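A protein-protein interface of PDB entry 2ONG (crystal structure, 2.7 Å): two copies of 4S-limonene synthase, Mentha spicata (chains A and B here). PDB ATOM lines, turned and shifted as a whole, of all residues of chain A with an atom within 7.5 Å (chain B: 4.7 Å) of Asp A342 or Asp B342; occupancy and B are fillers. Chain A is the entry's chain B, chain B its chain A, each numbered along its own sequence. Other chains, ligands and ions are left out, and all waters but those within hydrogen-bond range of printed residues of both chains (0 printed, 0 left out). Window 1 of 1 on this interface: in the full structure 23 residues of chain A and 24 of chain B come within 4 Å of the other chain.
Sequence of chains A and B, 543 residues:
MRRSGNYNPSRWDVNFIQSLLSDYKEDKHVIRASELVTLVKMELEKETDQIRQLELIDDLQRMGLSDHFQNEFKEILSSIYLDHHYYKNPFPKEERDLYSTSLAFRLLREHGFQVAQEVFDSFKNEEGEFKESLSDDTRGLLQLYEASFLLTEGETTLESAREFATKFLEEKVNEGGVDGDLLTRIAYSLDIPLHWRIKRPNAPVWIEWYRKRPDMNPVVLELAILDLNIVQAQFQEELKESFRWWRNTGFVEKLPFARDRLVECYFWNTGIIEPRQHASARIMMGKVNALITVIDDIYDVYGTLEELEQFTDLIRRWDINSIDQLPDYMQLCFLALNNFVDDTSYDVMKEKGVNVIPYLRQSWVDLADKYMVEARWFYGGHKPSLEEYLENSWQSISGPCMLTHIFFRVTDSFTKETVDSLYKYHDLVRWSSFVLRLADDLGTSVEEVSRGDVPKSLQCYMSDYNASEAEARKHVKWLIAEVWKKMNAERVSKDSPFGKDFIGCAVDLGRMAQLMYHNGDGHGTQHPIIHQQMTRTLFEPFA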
ATOM      1  N   TRP A 318      31.146  31.797   8.098  1.00  0.00           N
ATOM      2  CA  TRP A 318      29.816  31.404   8.455  1.00  0.00           C
ATOM      3  C   TRP A 318      28.656  31.609   7.495  1.00  0.00           C
ATOM      4  O   TRP A 318      27.879  32.565   7.643  1.00  0.00           O
ATOM      5  CB  TRP A 318      29.488  32.069   9.798  1.00  0.00           C
ATOM      6  CG  TRP A 318      28.409  31.287  10.543  1.00  0.00           C
ATOM      7  CD1 TRP A 318      27.075  31.323  10.199  1.00  0.00           C
ATOM      8  CD2 TRP A 318      28.601  30.493  11.619  1.00  0.00           C
ATOM      9  NE1 TRP A 318      26.399  30.521  11.093  1.00  0.00           N
ATOM     10  CE2 TRP A 318      27.322  30.042  11.919  1.00  0.00           C
ATOM     11  CE3 TRP A 318      29.681  30.102  12.364  1.00  0.00           C
ATOM     12  CZ2 TRP A 318      27.087  29.193  12.965  1.00  0.00           C
ATOM     13  CZ3 TRP A 318      29.451  29.231  13.435  1.00  0.00           C
ATOM     14  CH2 TRP A 318      28.167  28.782  13.733  1.00  0.00           C
ATOM     15  N   ILE A 320      25.570  29.407   5.319  1.00  0.00           N
ATOM     16  CA  ILE A 320      24.705  28.331   4.937  1.00  0.00           C
ATOM     17  C   ILE A 320      24.224  28.399   3.487  1.00  0.00           C
ATOM     18  O   ILE A 320      23.180  27.809   3.112  1.00  0.00           O
ATOM     19  CB  ILE A 320      23.472  28.301   5.832  1.00  0.00           C
ATOM     20  CG1 ILE A 320      23.032  29.764   5.946  1.00  0.00           C
ATOM     21  CG2 ILE A 320      23.739  27.649   7.173  1.00  0.00           C
ATOM     22  CD1 ILE A 320      23.096  30.351   7.374  1.00  0.00           C
ATOM     23  N   LEU A 335      25.424  22.665   9.516  1.00  0.00           N
ATOM     24  CA  LEU A 335      24.087  23.184   9.755  1.00  0.00           C
ATOM     25  C   LEU A 335      23.534  22.880  11.147  1.00  0.00           C
ATOM     26  O   LEU A 335      22.881  23.737  11.759  1.00  0.00           O
ATOM     27  CB  LEU A 335      23.115  22.636   8.701  1.00  0.00           C
ATOM     28  CG  LEU A 335      21.715  23.261   8.729  1.00  0.00           C
ATOM     29  CD1 LEU A 335      21.655  24.404   7.734  1.00  0.00           C
ATOM     30  CD2 LEU A 335      20.643  22.256   8.320  1.00  0.00           C
ATOM     31  N   ALA A 336      23.777  21.678  11.657  1.00  0.00           N
ATOM     32  CA  ALA A 336      23.183  21.546  12.970  1.00  0.00           C
ATOM     33  C   ALA A 336      23.877  22.465  13.959  1.00  0.00           C
ATOM     34  O   ALA A 336      23.226  23.009  14.871  1.00  0.00           O
ATOM     35  CB  ALA A 336      23.281  20.125  13.452  1.00  0.00           C
ATOM     36  N   LEU A 337      25.190  22.631  13.789  1.00  0.00           N
ATOM     37  CA  LEU A 337      25.976  23.495  14.675  1.00  0.00           C
ATOM     38  C   LEU A 337      25.392  24.898  14.517  1.00  0.00           C
ATOM     39  O   LEU A 337      25.173  25.567  15.506  1.00  0.00           O
ATOM     40  CB  LEU A 337      27.465  23.522  14.314  1.00  0.00           C
ATOM     41  CG  LEU A 337      28.231  24.816  14.593  1.00  0.00           C
ATOM     42  CD1 LEU A 337      28.405  25.060  16.088  1.00  0.00           C
ATOM     43  CD2 LEU A 337      29.680  24.623  14.295  1.00  0.00           C
ATOM     44  N   ASN A 338      25.133  25.348  13.293  1.00  0.00           N
ATOM     45  CA  ASN A 338      24.573  26.673  13.210  1.00  0.00           C
ATOM     46  C   ASN A 338      23.255  26.632  13.963  1.00  0.00           C
ATOM     47  O   ASN A 338      23.061  27.411  14.894  1.00  0.00           O
ATOM     48  CB  ASN A 338      24.306  27.108  11.775  1.00  0.00           C
ATOM     49  CG  ASN A 338      23.081  28.027  11.671  1.00  0.00           C
ATOM     50  OD1 ASN A 338      21.946  27.544  11.678  1.00  0.00           O
ATOM     51  ND2 ASN A 338      23.300  29.344  11.570  1.00  0.00           N
ATOM     52  N   ASN A 339      22.345  25.740  13.577  1.00  0.00           N
ATOM     53  CA  ASN A 339      21.061  25.697  14.300  1.00  0.00           C
ATOM     54  C   ASN A 339      21.143  25.835  15.830  1.00  0.00           C
ATOM     55  O   ASN A 339      20.350  26.535  16.442  1.00  0.00           O
ATOM     56  CB  ASN A 339      20.381  24.381  13.920  1.00  0.00           C
ATOM     57  CG  ASN A 339      19.831  24.278  12.511  1.00  0.00           C
ATOM     58  OD1 ASN A 339      19.076  23.356  12.204  1.00  0.00           O
ATOM     59  ND2 ASN A 339      20.201  25.216  11.648  1.00  0.00           N
ATOM     60  N   PHE A 340      22.111  25.165  16.446  1.00  0.00           N
ATOM     61  CA  PHE A 340      22.270  25.247  17.891  1.00  0.00           C
ATOM     62  C   PHE A 340      22.613  26.661  18.351  1.00  0.00           C
ATOM     63  O   PHE A 340      21.981  27.201  19.260  1.00  0.00           O
ATOM     64  CB  PHE A 340      23.375  24.278  18.294  1.00  0.00           C
ATOM     65  CG  PHE A 340      23.835  24.583  19.659  1.00  0.00           C
ATOM     66  CD1 PHE A 340      23.192  23.943  20.673  1.00  0.00           C
ATOM     67  CD2 PHE A 340      24.868  25.479  19.886  1.00  0.00           C
ATOM     68  CE1 PHE A 340      23.581  24.197  21.978  1.00  0.00           C
ATOM     69  CE2 PHE A 340      25.259  25.732  21.192  1.00  0.00           C
ATOM     70  CZ  PHE A 340      24.617  25.094  22.237  1.00  0.00           C
ATOM     71  N   VAL A 341      23.623  27.259  17.730  1.00  0.00           N
ATOM     72  CA  VAL A 341      23.833  28.564  18.253  1.00  0.00           C
ATOM     73  C   VAL A 341      22.570  29.380  18.048  1.00  0.00           C
ATOM     74  O   VAL A 341      22.196  30.156  18.925  1.00  0.00           O
ATOM     75  CB  VAL A 341      25.019  29.289  17.573  1.00  0.00           C
ATOM     76  CG1 VAL A 341      25.794  28.277  16.791  1.00  0.00           C
ATOM     77  CG2 VAL A 341      24.592  30.400  16.640  1.00  0.00           C
ATOM     78  N   ASP A 342      21.909  29.199  16.906  1.00  0.00           N
ATOM     79  CA  ASP A 342      20.694  29.950  16.592  1.00  0.00           C
ATOM     80  C   ASP A 342      19.645  29.596  17.627  1.00  0.00           C
ATOM     81  O   ASP A 342      18.861  30.459  18.063  1.00  0.00           O
ATOM     82  CB  ASP A 342      20.162  29.602  15.202  1.00  0.00           C
ATOM     83  CG  ASP A 342      20.738  30.352  14.010  1.00  0.00           C
ATOM     84  OD1 ASP A 342      21.751  31.079  14.175  1.00  0.00           O
ATOM     85  OD2 ASP A 342      20.161  30.193  12.905  1.00  0.00           O
ATOM     86  N   ASP A 343      19.631  28.335  18.042  1.00  0.00           N
ATOM     87  CA  ASP A 343      18.570  28.078  19.037  1.00  0.00           C
ATOM     88  C   ASP A 343      18.838  28.674  20.405  1.00  0.00           C
ATOM     89  O   ASP A 343      17.991  29.358  20.996  1.00  0.00           O
ATOM     90  CB  ASP A 343      18.343  26.585  19.221  1.00  0.00           C
ATOM     91  CG  ASP A 343      17.632  26.380  20.586  1.00  0.00           C
ATOM     92  OD1 ASP A 343      18.248  25.681  21.425  1.00  0.00           O
ATOM     93  OD2 ASP A 343      16.503  26.890  20.812  1.00  0.00           O
ATOM     94  N   THR A 344      20.038  28.376  20.890  1.00  0.00           N
ATOM     95  CA  THR A 344      20.543  28.797  22.119  1.00  0.00           C
ATOM     96  C   THR A 344      20.340  30.311  22.085  1.00  0.00           C
ATOM     97  O   THR A 344      19.720  30.894  23.002  1.00  0.00           O
ATOM     98  CB  THR A 344      22.000  28.344  22.231  1.00  0.00           C
ATOM     99  OG1 THR A 344      22.002  26.978  22.521  1.00  0.00           O
ATOM    100  CG2 THR A 344      22.784  29.083  23.293  1.00  0.00           C
ATOM    101  N   SER A 345      20.830  30.946  21.023  1.00  0.00           N
ATOM    102  CA  SER A 345      20.664  32.385  20.943  1.00  0.00           C
ATOM    103  C   SER A 345      19.230  32.884  21.004  1.00  0.00           C
ATOM    104  O   SER A 345      18.971  34.000  21.469  1.00  0.00           O
ATOM    105  CB  SER A 345      21.329  32.868  19.670  1.00  0.00           C
ATOM    106  OG  SER A 345      22.651  33.278  19.950  1.00  0.00           O
ATOM    107  N   TYR A 346      18.300  32.061  20.520  1.00  0.00           N
ATOM    108  CA  TYR A 346      16.921  32.527  20.607  1.00  0.00           C
ATOM    109  C   TYR A 346      16.516  32.445  22.072  1.00  0.00           C
ATOM    110  O   TYR A 346      15.737  33.236  22.523  1.00  0.00           O
ATOM    111  CB  TYR A 346      15.962  31.667  19.787  1.00  0.00           C
ATOM    112  CG  TYR A 346      14.517  32.185  19.827  1.00  0.00           C
ATOM    113  CD1 TYR A 346      14.114  33.208  18.986  1.00  0.00           C
ATOM    114  CD2 TYR A 346      13.574  31.611  20.671  1.00  0.00           C
ATOM    115  CE1 TYR A 346      12.795  33.655  18.974  1.00  0.00           C
ATOM    116  CE2 TYR A 346      12.240  32.059  20.661  1.00  0.00           C
ATOM    117  CZ  TYR A 346      11.881  33.077  19.808  1.00  0.00           C
ATOM    118  OH  TYR A 346      10.651  33.492  19.797  1.00  0.00           O
ATOM    119  N   ASP A 347      17.042  31.472  22.805  1.00  0.00           N
ATOM    120  CA  ASP A 347      16.675  31.388  24.183  1.00  0.00           C
ATOM    121  C   ASP A 347      17.204  32.581  24.963  1.00  0.00           C
ATOM    122  O   ASP A 347      16.489  33.186  25.721  1.00  0.00           O
ATOM    123  CB  ASP A 347      17.253  30.102  24.733  1.00  0.00           C
ATOM    124  CG  ASP A 347      16.272  29.053  24.357  1.00  0.00           C
ATOM    125  OD1 ASP A 347      16.451  27.890  24.782  1.00  0.00           O
ATOM    126  OD2 ASP A 347      15.313  29.396  23.636  1.00  0.00           O
ATOM    127  N   VAL A 348      18.474  32.905  24.769  1.00  0.00           N
ATOM    128  CA  VAL A 348      18.982  34.017  25.473  1.00  0.00           C
ATOM    129  C   VAL A 348      18.196  35.235  24.972  1.00  0.00           C
ATOM    130  O   VAL A 348      17.761  36.054  25.770  1.00  0.00           O
ATOM    131  CB  VAL A 348      20.499  34.150  25.223  1.00  0.00           C
ATOM    132  CG1 VAL A 348      21.103  35.472  25.662  1.00  0.00           C
ATOM    133  CG2 VAL A 348      21.133  33.040  26.047  1.00  0.00           C
ATOM    134  N   MET A 349      17.995  35.362  23.663  1.00  0.00           N
ATOM    135  CA  MET A 349      17.232  36.551  23.264  1.00  0.00           C
ATOM    136  C   MET A 349      15.840  36.612  23.878  1.00  0.00           C
ATOM    137  O   MET A 349      15.332  37.684  24.175  1.00  0.00           O
ATOM    138  CB  MET A 349      17.106  36.615  21.741  1.00  0.00           C
ATOM    139  CG  MET A 349      15.905  37.403  21.240  1.00  0.00           C
ATOM    140  SD  MET A 349      16.314  38.255  19.691  1.00  0.00           S
ATOM    141  CE  MET A 349      17.272  37.105  18.745  1.00  0.00           C
ATOM    142  N   ILE A 357      23.865  35.682  19.279  1.00  0.00           N
ATOM    143  CA  ILE A 357      24.408  34.839  18.231  1.00  0.00           C
ATOM    144  C   ILE A 357      25.774  35.226  17.688  1.00  0.00           C
ATOM    145  O   ILE A 357      26.577  34.356  17.387  1.00  0.00           O
ATOM    146  CB  ILE A 357      23.401  34.669  17.013  1.00  0.00           C
ATOM    147  CG1 ILE A 357      23.767  35.596  15.859  1.00  0.00           C
ATOM    148  CG2 ILE A 357      21.948  34.941  17.387  1.00  0.00           C
ATOM    149  CD1 ILE A 357      22.578  35.857  14.895  1.00  0.00           C
ATOM    150  N   LEU A 360      28.510  33.433  20.138  1.00  0.00           N
ATOM    151  CA  LEU A 360      28.626  31.996  20.278  1.00  0.00           C
ATOM    152  C   LEU A 360      29.184  31.569  18.925  1.00  0.00           C
ATOM    153  O   LEU A 360      30.024  30.655  18.833  1.00  0.00           O
ATOM    154  CB  LEU A 360      27.252  31.388  20.544  1.00  0.00           C
ATOM    155  CG  LEU A 360      26.699  31.878  21.881  1.00  0.00           C
ATOM    156  CD1 LEU A 360      25.214  31.605  22.016  1.00  0.00           C
ATOM    157  CD2 LEU A 360      27.424  31.152  22.989  1.00  0.00           C
ATOM    158  N   ARG A 361      28.728  32.256  17.881  1.00  0.00           N
ATOM    159  CA  ARG A 361      29.201  31.970  16.527  1.00  0.00           C
ATOM    160  C   ARG A 361      30.727  32.032  16.665  1.00  0.00           C
ATOM    161  O   ARG A 361      31.436  31.054  16.396  1.00  0.00           O
ATOM    162  CB  ARG A 361      28.707  33.070  15.591  1.00  0.00           C
ATOM    163  CG  ARG A 361      28.182  32.573  14.251  1.00  0.00           C
ATOM    164  CD  ARG A 361      26.665  32.732  14.145  1.00  0.00           C
ATOM    165  NE  ARG A 361      26.248  33.473  12.952  1.00  0.00           N
ATOM    166  CZ  ARG A 361      25.012  33.447  12.458  1.00  0.00           C
ATOM    167  NH1 ARG A 361      24.075  32.710  13.057  1.00  0.00           N
ATOM    168  NH2 ARG A 361      24.703  34.165  11.379  1.00  0.00           N
ATOM    169  N   LEU B 335      13.719  35.835  14.092  1.00  0.00           N
ATOM    170  CA  LEU B 335      14.642  34.749  14.404  1.00  0.00           C
ATOM    171  C   LEU B 335      13.801  33.493  14.589  1.00  0.00           C
ATOM    172  O   LEU B 335      14.237  32.407  14.199  1.00  0.00           O
ATOM    173  CB  LEU B 335      15.462  35.001  15.681  1.00  0.00           C
ATOM    174  CG  LEU B 335      16.765  34.197  15.831  1.00  0.00           C
ATOM    175  CD1 LEU B 335      17.969  35.091  15.633  1.00  0.00           C
ATOM    176  CD2 LEU B 335      17.022  33.808  17.271  1.00  0.00           C
ATOM    177  N   ASN B 338      13.632  32.302  11.119  1.00  0.00           N
ATOM    178  CA  ASN B 338      14.882  31.720  10.649  1.00  0.00           C
ATOM    179  C   ASN B 338      15.207  30.482  11.458  1.00  0.00           C
ATOM    180  O   ASN B 338      15.968  29.632  11.018  1.00  0.00           O
ATOM    181  CB  ASN B 338      16.048  32.702  10.768  1.00  0.00           C
ATOM    182  CG  ASN B 338      17.427  32.032  10.629  1.00  0.00           C
ATOM    183  OD1 ASN B 338      18.052  32.060   9.545  1.00  0.00           O
ATOM    184  ND2 ASN B 338      17.905  31.432  11.719  1.00  0.00           N
ATOM    185  N   ASN B 339      14.632  30.379  12.647  1.00  0.00           N
ATOM    186  CA  ASN B 339      15.008  29.178  13.325  1.00  0.00           C
ATOM    187  C   ASN B 339      14.208  28.011  12.759  1.00  0.00           C
ATOM    188  O   ASN B 339      14.740  26.912  12.592  1.00  0.00           O
ATOM    189  CB  ASN B 339      14.735  29.369  14.810  1.00  0.00           C
ATOM    190  CG  ASN B 339      16.010  29.843  15.482  1.00  0.00           C
ATOM    191  OD1 ASN B 339      16.964  30.269  14.818  1.00  0.00           O
ATOM    192  ND2 ASN B 339      16.032  29.769  16.812  1.00  0.00           N
ATOM    193  N   PHE B 340      12.933  28.256  12.456  1.00  0.00           N
ATOM    194  CA  PHE B 340      12.029  27.242  11.891  1.00  0.00           C
ATOM    195  C   PHE B 340      12.477  26.789  10.507  1.00  0.00           C
ATOM    196  O   PHE B 340      12.595  25.599  10.276  1.00  0.00           O
ATOM    197  CB  PHE B 340      10.596  27.777  11.796  1.00  0.00           C
ATOM    198  CG  PHE B 340       9.761  26.806  10.991  1.00  0.00           C
ATOM    199  CD1 PHE B 340       9.240  25.697  11.629  1.00  0.00           C
ATOM    200  CD2 PHE B 340       9.555  27.017   9.631  1.00  0.00           C
ATOM    201  CE1 PHE B 340       8.502  24.768  10.903  1.00  0.00           C
ATOM    202  CE2 PHE B 340       8.811  26.082   8.897  1.00  0.00           C
ATOM    203  CZ  PHE B 340       8.288  24.961   9.535  1.00  0.00           C
ATOM    204  N   VAL B 341      12.726  27.715   9.585  1.00  0.00           N
ATOM    205  CA  VAL B 341      13.122  27.058   8.370  1.00  0.00           C
ATOM    206  C   VAL B 341      14.413  26.275   8.504  1.00  0.00           C
ATOM    207  O   VAL B 341      14.561  25.242   7.881  1.00  0.00           O
ATOM    208  CB  VAL B 341      13.300  28.043   7.204  1.00  0.00           C
ATOM    209  CG1 VAL B 341      12.291  29.138   7.433  1.00  0.00           C
ATOM    210  CG2 VAL B 341      14.735  28.481   7.044  1.00  0.00           C
ATOM    211  N   ASP B 342      15.337  26.764   9.328  1.00  0.00           N
ATOM    212  CA  ASP B 342      16.588  26.063   9.475  1.00  0.00           C
ATOM    213  C   ASP B 342      16.405  24.711  10.154  1.00  0.00           C
ATOM    214  O   ASP B 342      17.037  23.719   9.752  1.00  0.00           O
ATOM    215  CB  ASP B 342      17.552  26.940  10.270  1.00  0.00           C
ATOM    216  CG  ASP B 342      18.162  28.074   9.422  1.00  0.00           C
ATOM    217  OD1 ASP B 342      17.720  28.208   8.259  1.00  0.00           O
ATOM    218  OD2 ASP B 342      19.061  28.813   9.904  1.00  0.00           O
ATOM    219  N   ASP B 343      15.550  24.648  11.175  1.00  0.00           N
ATOM    220  CA  ASP B 343      15.407  23.323  11.789  1.00  0.00           C
ATOM    221  C   ASP B 343      14.616  22.445  10.828  1.00  0.00           C
ATOM    222  O   ASP B 343      14.825  21.229  10.774  1.00  0.00           O
ATOM    223  CB  ASP B 343      14.668  23.341  13.132  1.00  0.00           C
ATOM    224  CG  ASP B 343      13.977  21.950  13.414  1.00  0.00           C
ATOM    225  OD1 ASP B 343      12.734  21.846  13.273  1.00  0.00           O
ATOM    226  OD2 ASP B 343      14.688  20.979  13.768  1.00  0.00           O
ATOM    227  N   THR B 344      13.699  23.052  10.080  1.00  0.00           N
ATOM    228  CA  THR B 344      12.969  22.225   9.172  1.00  0.00           C
ATOM    229  C   THR B 344      13.900  21.803   8.035  1.00  0.00           C
ATOM    230  O   THR B 344      13.980  20.620   7.719  1.00  0.00           O
ATOM    231  CB  THR B 344      11.742  22.965   8.663  1.00  0.00           C
ATOM    232  OG1 THR B 344      10.677  22.729   9.552  1.00  0.00           O
ATOM    233  CG2 THR B 344      11.351  22.504   7.285  1.00  0.00           C
ATOM    234  N   SER B 345      14.621  22.744   7.433  1.00  0.00           N
ATOM    235  CA  SER B 345      15.480  22.252   6.382  1.00  0.00           C
ATOM    236  C   SER B 345      16.555  21.270   6.830  1.00  0.00           C
ATOM    237  O   SER B 345      17.138  20.580   5.992  1.00  0.00           O
ATOM    238  CB  SER B 345      16.135  23.421   5.662  1.00  0.00           C
ATOM    239  OG  SER B 345      15.237  24.505   5.563  1.00  0.00           O
ATOM    240  N   TYR B 346      16.824  21.212   8.136  1.00  0.00           N
ATOM    241  CA  TYR B 346      17.828  20.286   8.673  1.00  0.00           C
ATOM    242  C   TYR B 346      17.196  18.908   8.509  1.00  0.00           C
ATOM    243  O   TYR B 346      17.818  18.023   7.960  1.00  0.00           O
ATOM    244  CB  TYR B 346      18.110  20.548  10.154  1.00  0.00           C
ATOM    245  CG  TYR B 346      19.120  19.540  10.658  1.00  0.00           C
ATOM    246  CD1 TYR B 346      20.483  19.760  10.409  1.00  0.00           C
ATOM    247  CD2 TYR B 346      18.684  18.404  11.342  1.00  0.00           C
ATOM    248  CE1 TYR B 346      21.429  18.844  10.833  1.00  0.00           C
ATOM    249  CE2 TYR B 346      19.633  17.472  11.779  1.00  0.00           C
ATOM    250  CZ  TYR B 346      20.978  17.718  11.505  1.00  0.00           C
ATOM    251  OH  TYR B 346      21.840  16.814  11.856  1.00  0.00           O
ATOM    252  N   ILE B 357      16.838  24.861   2.453  1.00  0.00           N
ATOM    253  CA  ILE B 357      16.666  26.208   2.977  1.00  0.00           C
ATOM    254  C   ILE B 357      16.557  27.360   2.002  1.00  0.00           C
ATOM    255  O   ILE B 357      16.058  28.411   2.357  1.00  0.00           O
ATOM    256  CB  ILE B 357      17.800  26.643   3.959  1.00  0.00           C
ATOM    257  CG1 ILE B 357      18.898  27.347   3.160  1.00  0.00           C
ATOM    258  CG2 ILE B 357      18.357  25.474   4.743  1.00  0.00           C
ATOM    259  CD1 ILE B 357      20.302  27.324   3.823  1.00  0.00           C
ATOM    260  N   ARG B 361      12.908  29.454   2.554  1.00  0.00           N
ATOM    261  CA  ARG B 361      13.261  30.829   2.791  1.00  0.00           C
ATOM    262  C   ARG B 361      12.426  31.674   1.823  1.00  0.00           C
ATOM    263  O   ARG B 361      11.677  32.545   2.256  1.00  0.00           O
ATOM    264  CB  ARG B 361      14.748  31.019   2.519  1.00  0.00           C
ATOM    265  CG  ARG B 361      15.419  32.001   3.457  1.00  0.00           C
ATOM    266  CD  ARG B 361      16.320  31.315   4.474  1.00  0.00           C
ATOM    267  NE  ARG B 361      17.705  31.762   4.342  1.00  0.00           N
ATOM    268  CZ  ARG B 361      18.658  31.539   5.243  1.00  0.00           C
ATOM    269  NH1 ARG B 361      18.377  30.869   6.356  1.00  0.00           N
ATOM    270  NH2 ARG B 361      19.892  31.981   5.030  1.00  0.00           N
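The side-chain amide nitrogen of Asn B338 sits at hydrogen-bond distance from the side-chain carboxylate of Asp A342 (2.8 Å).
ND2 of Asn B339 sits at hydrogen-bond distance from O of Asp A342, 3.2 Å away.
O of Asp B342 lies close to OD1 of Asn A339, 3.2 Å away.
The side-chain carboxylate (OD2) of Asp A342 lies close to the side-chain carboxylate (OD2) of Asp B342 (3.5 Å).
ND2 of Asn B338 lies within hydrogen-bond range of OD1 of Asn B339 (3.4 Å).
The guanidinium group (NH1) of Arg B361 is in hydrogen-bond range of the side-chain amide oxygen (OD1) of Asn B338.
NE1 of Trp A318 lies close to ND2 of Asn A338 (3.3 Å).
The backbone carbonyl oxygen of Leu A335 is in hydrogen-bond range of the side-chain amide nitrogen of Asn A339.
The side-chain amide oxygen of Asn A338 lies within hydrogen-bond range of the side-chain amide nitrogen of Asn A339 (2.9 Å).
The guanidinium group of Arg A361 lies within salt-bridge range of the side-chain carboxylate of Asp A342 (3.1 Å).
O of Ile A320 touches CD1 of Ile B357, 3.0 Å away.
Leu A335 touches Tyr B346 (CD2 to CD1, 3.3 Å).
Tyr B346 touches Ala A336.
OD1 of Asn A338 touches OD2 of Asp B342, at 3.6 Å.
Asp B343 touches Asn A339 (CA to OD1, 3.7 Å).
Asn A339 touches Tyr B346.
Asp A342 touches Leu B335 (O to CD2, 3.9 Å).
CA of Asp A343 touches ND2 of Asn B339 (3.8 Å).
CD2 of Leu B335 touches CD1 of Tyr A346, 3.4 Å away.
CB of Tyr A346 touches ND2 of Asn B339, at 3.5 Å.
Printed residues of chain B within 4 Å of Ile A320: Ile B357 (3.0 Å) and Arg B361 (3.95 Å).
Printed residues of chain B within 4 Å of Asn A338: Asp B342 (3.6 Å).
Of chain B, only Leu B335, Asn B338, Asn B339 and Asp B342 come within 4 Å of Asp A342.
Printed residues of chain B within 4 Å of Tyr A346: Leu B335 and Asn B339.
Asp A347 touches none of the printed residues of chain B.
Of the printed residues of chain B, Met A349 touches Leu B335.
Of chain A, only Asn A338, Asn A339 and Asp A342 come within 4 Å of Asp B342.
The nearest printed residue of chain B that does not touch Asp A342 is Arg B361 (6.8 Å).
Hydrophobic or aromatic side chains of chain A that line the printed part of chain B: Ile A320, Leu A335, Ala A336, Tyr A346 and Met A349.
Printed residues of chain B that touch a printed residue of chain A: Leu B335, Asn B338, Asn B339, Asp B342, Asp B343, Tyr B346, Ile B357 and Arg B361.
Hydrophobic or aromatic side chains of chain B that line the printed part of chain A: Leu B335, Tyr B346 and Ile B357.
Among the printed residues, 16 pairs touch across the chains.
Asn A338 touches Asp B342, and with the chains exchanged Asp A342 touches Asn B338.
Asn A339 touches Asp B342, and with the chains exchanged Asp A342 touches Asn B339.
Asn A339 touches Asp B343, and with the chains exchanged Asp A343 touches Asn B339.
Asp A342 touches its own counterpart, Asp B342.
12 positions are printed for both chains.
Of the 16 pairs that touch across the chains among the printed residues, 11 have their exchanged pair printed and touching as well.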
